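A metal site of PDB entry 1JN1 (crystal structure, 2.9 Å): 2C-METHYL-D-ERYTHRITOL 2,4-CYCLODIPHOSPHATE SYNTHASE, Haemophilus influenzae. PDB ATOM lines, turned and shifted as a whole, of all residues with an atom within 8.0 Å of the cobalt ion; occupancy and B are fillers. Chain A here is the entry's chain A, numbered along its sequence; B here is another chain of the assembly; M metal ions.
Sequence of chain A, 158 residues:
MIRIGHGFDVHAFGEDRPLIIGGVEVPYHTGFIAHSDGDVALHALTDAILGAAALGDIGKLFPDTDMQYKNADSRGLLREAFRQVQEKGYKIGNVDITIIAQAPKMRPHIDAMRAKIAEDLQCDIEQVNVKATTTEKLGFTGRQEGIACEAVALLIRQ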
ATOM      1  N   PHE A   8      -7.486 -18.485 -17.362  1.00  0.00           N
ATOM      2  CA  PHE A   8      -6.197 -18.267 -17.961  1.00  0.00           C
ATOM      3  C   PHE A   8      -5.082 -18.272 -16.918  1.00  0.00           C
ATOM      4  O   PHE A   8      -5.292 -17.782 -15.824  1.00  0.00           O
ATOM      5  CB  PHE A   8      -6.301 -16.926 -18.684  1.00  0.00           C
ATOM      6  CG  PHE A   8      -5.005 -16.351 -19.072  1.00  0.00           C
ATOM      7  CD1 PHE A   8      -4.369 -16.758 -20.226  1.00  0.00           C
ATOM      8  CD2 PHE A   8      -4.443 -15.356 -18.313  1.00  0.00           C
ATOM      9  CE1 PHE A   8      -3.194 -16.171 -20.627  1.00  0.00           C
ATOM     10  CE2 PHE A   8      -3.281 -14.774 -18.712  1.00  0.00           C
ATOM     11  CZ  PHE A   8      -2.648 -15.172 -19.869  1.00  0.00           C
ATOM     12  N   ASP A   9      -3.902 -18.827 -17.235  1.00  0.00           N
ATOM     13  CA  ASP A   9      -2.784 -18.885 -16.287  1.00  0.00           C
ATOM     14  C   ASP A   9      -1.425 -18.821 -16.923  1.00  0.00           C
ATOM     15  O   ASP A   9      -1.168 -19.435 -17.969  1.00  0.00           O
ATOM     16  CB  ASP A   9      -2.844 -20.155 -15.477  1.00  0.00           C
ATOM     17  CG  ASP A   9      -2.296 -19.992 -14.087  1.00  0.00           C
ATOM     18  OD1 ASP A   9      -2.100 -21.051 -13.455  1.00  0.00           O
ATOM     19  OD2 ASP A   9      -2.072 -18.855 -13.594  1.00  0.00           O
ATOM     20  N   VAL A  10      -0.558 -18.053 -16.279  1.00  0.00           N
ATOM     21  CA  VAL A  10       0.797 -17.887 -16.741  1.00  0.00           C
ATOM     22  C   VAL A  10       1.726 -18.313 -15.629  1.00  0.00           C
ATOM     23  O   VAL A  10       1.488 -18.008 -14.475  1.00  0.00           O
ATOM     24  CB  VAL A  10       1.099 -16.433 -17.072  1.00  0.00           C
ATOM     25  CG1 VAL A  10       2.589 -16.249 -17.106  1.00  0.00           C
ATOM     26  CG2 VAL A  10       0.502 -16.044 -18.413  1.00  0.00           C
ATOM     27  N   HIS A  11       2.779 -19.062 -15.921  1.00  0.00           N
ATOM     28  CA  HIS A  11       3.704 -19.412 -14.850  1.00  0.00           C
ATOM     29  C   HIS A  11       5.119 -19.378 -15.305  1.00  0.00           C
ATOM     30  O   HIS A  11       5.421 -19.779 -16.420  1.00  0.00           O
ATOM     31  CB  HIS A  11       3.453 -20.815 -14.297  1.00  0.00           C
ATOM     32  CG  HIS A  11       2.517 -20.852 -13.135  1.00  0.00           C
ATOM     33  ND1 HIS A  11       2.814 -20.275 -11.922  1.00  0.00           N
ATOM     34  CD2 HIS A  11       1.296 -21.400 -13.001  1.00  0.00           C
ATOM     35  CE1 HIS A  11       1.815 -20.462 -11.091  1.00  0.00           C
ATOM     36  NE2 HIS A  11       0.871 -21.144 -11.720  1.00  0.00           N
ATOM     37  N   HIS A  29       1.028 -13.230  -3.299  1.00  0.00           N
ATOM     38  CA  HIS A  29      -0.216 -12.790  -3.860  1.00  0.00           C
ATOM     39  C   HIS A  29      -1.216 -13.755  -3.214  1.00  0.00           C
ATOM     40  O   HIS A  29      -0.829 -14.520  -2.319  1.00  0.00           O
ATOM     41  CB  HIS A  29      -0.196 -12.831  -5.409  1.00  0.00           C
ATOM     42  CG  HIS A  29      -0.179 -14.207  -6.008  1.00  0.00           C
ATOM     43  ND1 HIS A  29       0.824 -14.642  -6.864  1.00  0.00           N
ATOM     44  CD2 HIS A  29      -1.067 -15.235  -5.935  1.00  0.00           C
ATOM     45  CE1 HIS A  29       0.547 -15.858  -7.288  1.00  0.00           C
ATOM     46  NE2 HIS A  29      -0.597 -16.247  -6.743  1.00  0.00           N
ATOM     47  N   GLY A  31      -3.899 -16.530  -4.362  1.00  0.00           N
ATOM     48  CA  GLY A  31      -3.933 -17.981  -4.475  1.00  0.00           C
ATOM     49  C   GLY A  31      -2.508 -18.471  -4.706  1.00  0.00           C
ATOM     50  O   GLY A  31      -2.285 -19.419  -5.449  1.00  0.00           O
ATOM     51  N   PHE A  32      -1.547 -17.814  -4.076  1.00  0.00           N
ATOM     52  CA  PHE A  32      -0.161 -18.176  -4.282  1.00  0.00           C
ATOM     53  C   PHE A  32       0.265 -19.595  -3.998  1.00  0.00           C
ATOM     54  O   PHE A  32       0.948 -20.180  -4.824  1.00  0.00           O
ATOM     55  CB  PHE A  32       0.779 -17.289  -3.512  1.00  0.00           C
ATOM     56  CG  PHE A  32       2.207 -17.631  -3.747  1.00  0.00           C
ATOM     57  CD1 PHE A  32       2.931 -17.013  -4.774  1.00  0.00           C
ATOM     58  CD2 PHE A  32       2.806 -18.653  -3.010  1.00  0.00           C
ATOM     59  CE1 PHE A  32       4.241 -17.419  -5.049  1.00  0.00           C
ATOM     60  CE2 PHE A  32       4.095 -19.042  -3.276  1.00  0.00           C
ATOM     61  CZ  PHE A  32       4.817 -18.438  -4.306  1.00  0.00           C
ATOM     62  N   ALA A  34      -1.691 -22.399  -3.646  1.00  0.00           N
ATOM     63  CA  ALA A  34      -2.380 -23.328  -4.556  1.00  0.00           C
ATOM     64  C   ALA A  34      -1.748 -23.394  -5.978  1.00  0.00           C
ATOM     65  O   ALA A  34      -1.705 -24.468  -6.592  1.00  0.00           O
ATOM     66  CB  ALA A  34      -3.871 -22.943  -4.656  1.00  0.00           C
ATOM     67  N   HIS A  35      -1.263 -22.258  -6.470  1.00  0.00           N
ATOM     68  CA  HIS A  35      -0.634 -22.123  -7.765  1.00  0.00           C
ATOM     69  C   HIS A  35       0.822 -22.621  -7.754  1.00  0.00           C
ATOM     70  O   HIS A  35       1.311 -23.076  -8.760  1.00  0.00           O
ATOM     71  CB  HIS A  35      -0.590 -20.645  -8.204  1.00  0.00           C
ATOM     72  CG  HIS A  35      -1.879 -20.105  -8.746  1.00  0.00           C
ATOM     73  ND1 HIS A  35      -2.287 -20.306 -10.055  1.00  0.00           N
ATOM     74  CD2 HIS A  35      -2.885 -19.409  -8.161  1.00  0.00           C
ATOM     75  CE1 HIS A  35      -3.472 -19.772 -10.237  1.00  0.00           C
ATOM     76  NE2 HIS A  35      -3.868 -19.223  -9.105  1.00  0.00           N
ATOM     77  N   SER A  36       1.514 -22.495  -6.626  1.00  0.00           N
ATOM     78  CA  SER A  36       2.948 -22.883  -6.496  1.00  0.00           C
ATOM     79  C   SER A  36       3.435 -24.051  -7.350  1.00  0.00           C
ATOM     80  O   SER A  36       4.586 -24.069  -7.761  1.00  0.00           O
ATOM     81  CB  SER A  36       3.326 -23.145  -5.036  1.00  0.00           C
ATOM     82  OG  SER A  36       2.509 -24.158  -4.498  1.00  0.00           O
ATOM     83  N   ASP A  37       2.550 -25.010  -7.552  1.00  0.00           N
ATOM     84  CA  ASP A  37       2.712 -26.212  -8.362  1.00  0.00           C
ATOM     85  C   ASP A  37       3.120 -25.706  -9.795  1.00  0.00           C
ATOM     86  O   ASP A  37       4.059 -26.186 -10.430  1.00  0.00           O
ATOM     87  CB  ASP A  37       1.314 -26.826  -8.267  1.00  0.00           C
ATOM     88  CG  ASP A  37       1.166 -28.106  -8.981  1.00  0.00           C
ATOM     89  OD1 ASP A  37       1.292 -28.098 -10.180  1.00  0.00           O
ATOM     90  OD2 ASP A  37       0.870 -29.113  -8.342  1.00  0.00           O
ATOM     91  N   GLY A  38       2.409 -24.691 -10.271  1.00  0.00           N
ATOM     92  CA  GLY A  38       2.686 -24.102 -11.562  1.00  0.00           C
ATOM     93  C   GLY A  38       2.150 -24.897 -12.744  1.00  0.00           C
ATOM     94  O   GLY A  38       2.642 -24.810 -13.868  1.00  0.00           O
ATOM     95  N   ASP A  39       1.088 -25.630 -12.517  1.00  0.00           N
ATOM     96  CA  ASP A  39       0.517 -26.445 -13.544  1.00  0.00           C
ATOM     97  C   ASP A  39      -0.568 -25.594 -14.172  1.00  0.00           C
ATOM     98  O   ASP A  39      -1.718 -25.723 -13.794  1.00  0.00           O
ATOM     99  CB  ASP A  39       0.009 -27.633 -12.767  1.00  0.00           C
ATOM    100  CG  ASP A  39      -0.374 -28.816 -13.604  1.00  0.00           C
ATOM    101  OD1 ASP A  39      -0.182 -29.915 -13.085  1.00  0.00           O
ATOM    102  OD2 ASP A  39      -0.877 -28.638 -14.711  1.00  0.00           O
ATOM    103  N   VAL A  40      -0.190 -24.699 -15.078  1.00  0.00           N
ATOM    104  CA  VAL A  40      -1.147 -23.797 -15.750  1.00  0.00           C
ATOM    105  C   VAL A  40      -2.301 -24.539 -16.355  1.00  0.00           C
ATOM    106  O   VAL A  40      -3.367 -23.981 -16.551  1.00  0.00           O
ATOM    107  CB  VAL A  40      -0.488 -23.016 -16.921  1.00  0.00           C
ATOM    108  CG1 VAL A  40       0.453 -21.930 -16.409  1.00  0.00           C
ATOM    109  CG2 VAL A  40       0.278 -24.018 -17.841  1.00  0.00           C
ATOM    110  N   ALA A  41      -2.130 -25.824 -16.639  1.00  0.00           N
ATOM    111  CA  ALA A  41      -3.216 -26.540 -17.288  1.00  0.00           C
ATOM    112  C   ALA A  41      -4.316 -26.853 -16.366  1.00  0.00           C
ATOM    113  O   ALA A  41      -5.483 -26.612 -16.668  1.00  0.00           O
ATOM    114  CB  ALA A  41      -2.706 -27.815 -17.913  1.00  0.00           C
ATOM    115  N   LEU A  42      -3.935 -27.390 -15.225  1.00  0.00           N
ATOM    116  CA  LEU A  42      -4.935 -27.770 -14.257  1.00  0.00           C
ATOM    117  C   LEU A  42      -5.532 -26.553 -13.592  1.00  0.00           C
ATOM    118  O   LEU A  42      -6.782 -26.498 -13.387  1.00  0.00           O
ATOM    119  CB  LEU A  42      -4.320 -28.753 -13.250  1.00  0.00           C
ATOM    120  CG  LEU A  42      -3.761 -30.089 -13.847  1.00  0.00           C
ATOM    121  CD1 LEU A  42      -3.125 -30.865 -12.759  1.00  0.00           C
ATOM    122  CD2 LEU A  42      -4.857 -30.935 -14.499  1.00  0.00           C
ATOM    123  N   HIS A  43      -4.697 -25.524 -13.323  1.00  0.00           N
ATOM    124  CA  HIS A  43      -5.196 -24.321 -12.652  1.00  0.00           C
ATOM    125  C   HIS A  43      -6.197 -23.545 -13.477  1.00  0.00           C
ATOM    126  O   HIS A  43      -7.188 -23.041 -12.940  1.00  0.00           O
ATOM    127  CB  HIS A  43      -4.067 -23.350 -12.220  1.00  0.00           C
ATOM    128  CG  HIS A  43      -3.050 -23.959 -11.293  1.00  0.00           C
ATOM    129  ND1 HIS A  43      -1.765 -23.459 -11.173  1.00  0.00           N
ATOM    130  CD2 HIS A  43      -3.077 -25.066 -10.514  1.00  0.00           C
ATOM    131  CE1 HIS A  43      -1.058 -24.235 -10.382  1.00  0.00           C
ATOM    132  NE2 HIS A  43      -1.830 -25.228  -9.976  1.00  0.00           N
ATOM    133  N   ALA A  44      -5.888 -23.412 -14.774  1.00  0.00           N
ATOM    134  CA  ALA A  44      -6.708 -22.664 -15.707  1.00  0.00           C
ATOM    135  C   ALA A  44      -8.027 -23.345 -15.880  1.00  0.00           C
ATOM    136  O   ALA A  44      -9.063 -22.696 -15.845  1.00  0.00           O
ATOM    137  CB  ALA A  44      -6.013 -22.561 -17.012  1.00  0.00           C
ATOM    138  N   ASP A  47     -10.041 -22.758 -12.890  1.00  0.00           N
ATOM    139  CA  ASP A  47     -10.553 -21.430 -12.960  1.00  0.00           C
ATOM    140  C   ASP A  47     -11.748 -21.420 -13.885  1.00  0.00           C
ATOM    141  O   ASP A  47     -12.692 -20.706 -13.633  1.00  0.00           O
ATOM    142  CB  ASP A  47      -9.464 -20.515 -13.529  1.00  0.00           C
ATOM    143  CG  ASP A  47      -8.792 -19.637 -12.476  1.00  0.00           C
ATOM    144  OD1 ASP A  47      -8.901 -19.917 -11.262  1.00  0.00           O
ATOM    145  OD2 ASP A  47      -8.141 -18.636 -12.908  1.00  0.00           O
ATOM    146  N   ILE A  58      -9.786 -19.763  -8.227  1.00  0.00           N
ATOM    147  CA  ILE A  58      -8.808 -20.406  -7.350  1.00  0.00           C
ATOM    148  C   ILE A  58      -8.301 -19.621  -6.127  1.00  0.00           C
ATOM    149  O   ILE A  58      -7.971 -20.224  -5.115  1.00  0.00           O
ATOM    150  CB  ILE A  58      -7.586 -20.826  -8.172  1.00  0.00           C
ATOM    151  CG1 ILE A  58      -7.922 -22.074  -8.957  1.00  0.00           C
ATOM    152  CG2 ILE A  58      -6.377 -21.054  -7.271  1.00  0.00           C
ATOM    153  CD1 ILE A  58      -6.745 -22.528  -9.821  1.00  0.00           C
ATOM    154  N   SER A  74      -2.318 -29.786  -7.283  1.00  0.00           N
ATOM    155  CA  SER A  74      -3.354 -29.130  -8.076  1.00  0.00           C
ATOM    156  C   SER A  74      -4.381 -30.018  -8.736  1.00  0.00           C
ATOM    157  O   SER A  74      -5.344 -29.533  -9.286  1.00  0.00           O
ATOM    158  CB  SER A  74      -2.737 -28.155  -9.088  1.00  0.00           C
ATOM    159  OG  SER A  74      -2.016 -28.841 -10.060  1.00  0.00           O
ATOM    160  N   THR B 133      -6.181 -12.699 -11.890  1.00  0.00           N
ATOM    161  CA  THR B 133      -4.862 -13.411 -11.796  1.00  0.00           C
ATOM    162  C   THR B 133      -3.724 -12.539 -12.217  1.00  0.00           C
ATOM    163  O   THR B 133      -3.903 -11.506 -12.848  1.00  0.00           O
ATOM    164  CB  THR B 133      -4.625 -14.518 -12.763  1.00  0.00           C
ATOM    165  OG1 THR B 133      -5.025 -14.075 -14.059  1.00  0.00           O
ATOM    166  CG2 THR B 133      -5.289 -15.797 -12.329  1.00  0.00           C
ATOM    167  N   THR B 134      -2.538 -13.029 -11.937  1.00  0.00           N
ATOM    168  CA  THR B 134      -1.308 -12.328 -12.271  1.00  0.00           C
ATOM    169  C   THR B 134      -0.581 -13.233 -13.260  1.00  0.00           C
ATOM    170  O   THR B 134      -0.907 -14.430 -13.393  1.00  0.00           O
ATOM    171  CB  THR B 134      -0.435 -12.144 -11.033  1.00  0.00           C
ATOM    172  OG1 THR B 134       0.408 -13.282 -10.888  1.00  0.00           O
ATOM    173  CG2 THR B 134      -1.301 -12.031  -9.749  1.00  0.00           C
ATOM    174  N   GLU B 136       2.626 -13.974 -13.126  1.00  0.00           N
ATOM    175  CA  GLU B 136       3.886 -14.244 -12.449  1.00  0.00           C
ATOM    176  C   GLU B 136       5.044 -13.455 -13.043  1.00  0.00           C
ATOM    177  O   GLU B 136       6.085 -14.017 -13.404  1.00  0.00           O
ATOM    178  CB  GLU B 136       4.155 -15.748 -12.496  1.00  0.00           C
ATOM    179  CG  GLU B 136       5.295 -16.208 -11.654  1.00  0.00           C
ATOM    180  CD  GLU B 136       5.224 -17.690 -11.332  1.00  0.00           C
ATOM    181  OE1 GLU B 136       6.229 -18.298 -10.898  1.00  0.00           O
ATOM    182  OE2 GLU B 136       4.146 -18.252 -11.526  1.00  0.00           O
HETATM  183 CO    CO M   1      -1.305 -21.411 -11.630  1.00  0.00          CO
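The cobalt ion is bound by the side-chain carboxylate (OD1) of Asp 9, a ring nitrogen (ND1) of His 43, a ring nitrogen (ND1) of His 35 and a ring nitrogen (NE2) of His 11.
A ring nitrogen (ND1) of His 11 lies within hydrogen-bond range of the side-chain carboxylate (OE2) of Glu 136 of chain B (2.5 Å). The backbone carbonyl oxygen (O) of Asp 39 lies close to a ring nitrogen (ND1) of His 43, 3.5 Å away. NE2 of His 43 is in hydrogen-bond range of O of Ala 34.
Of the 24 residues printed, 4 come within 4 Å of the cobalt ion. Along chain A the residues within 4 Å of the cobalt ion span positions 9 to 43.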
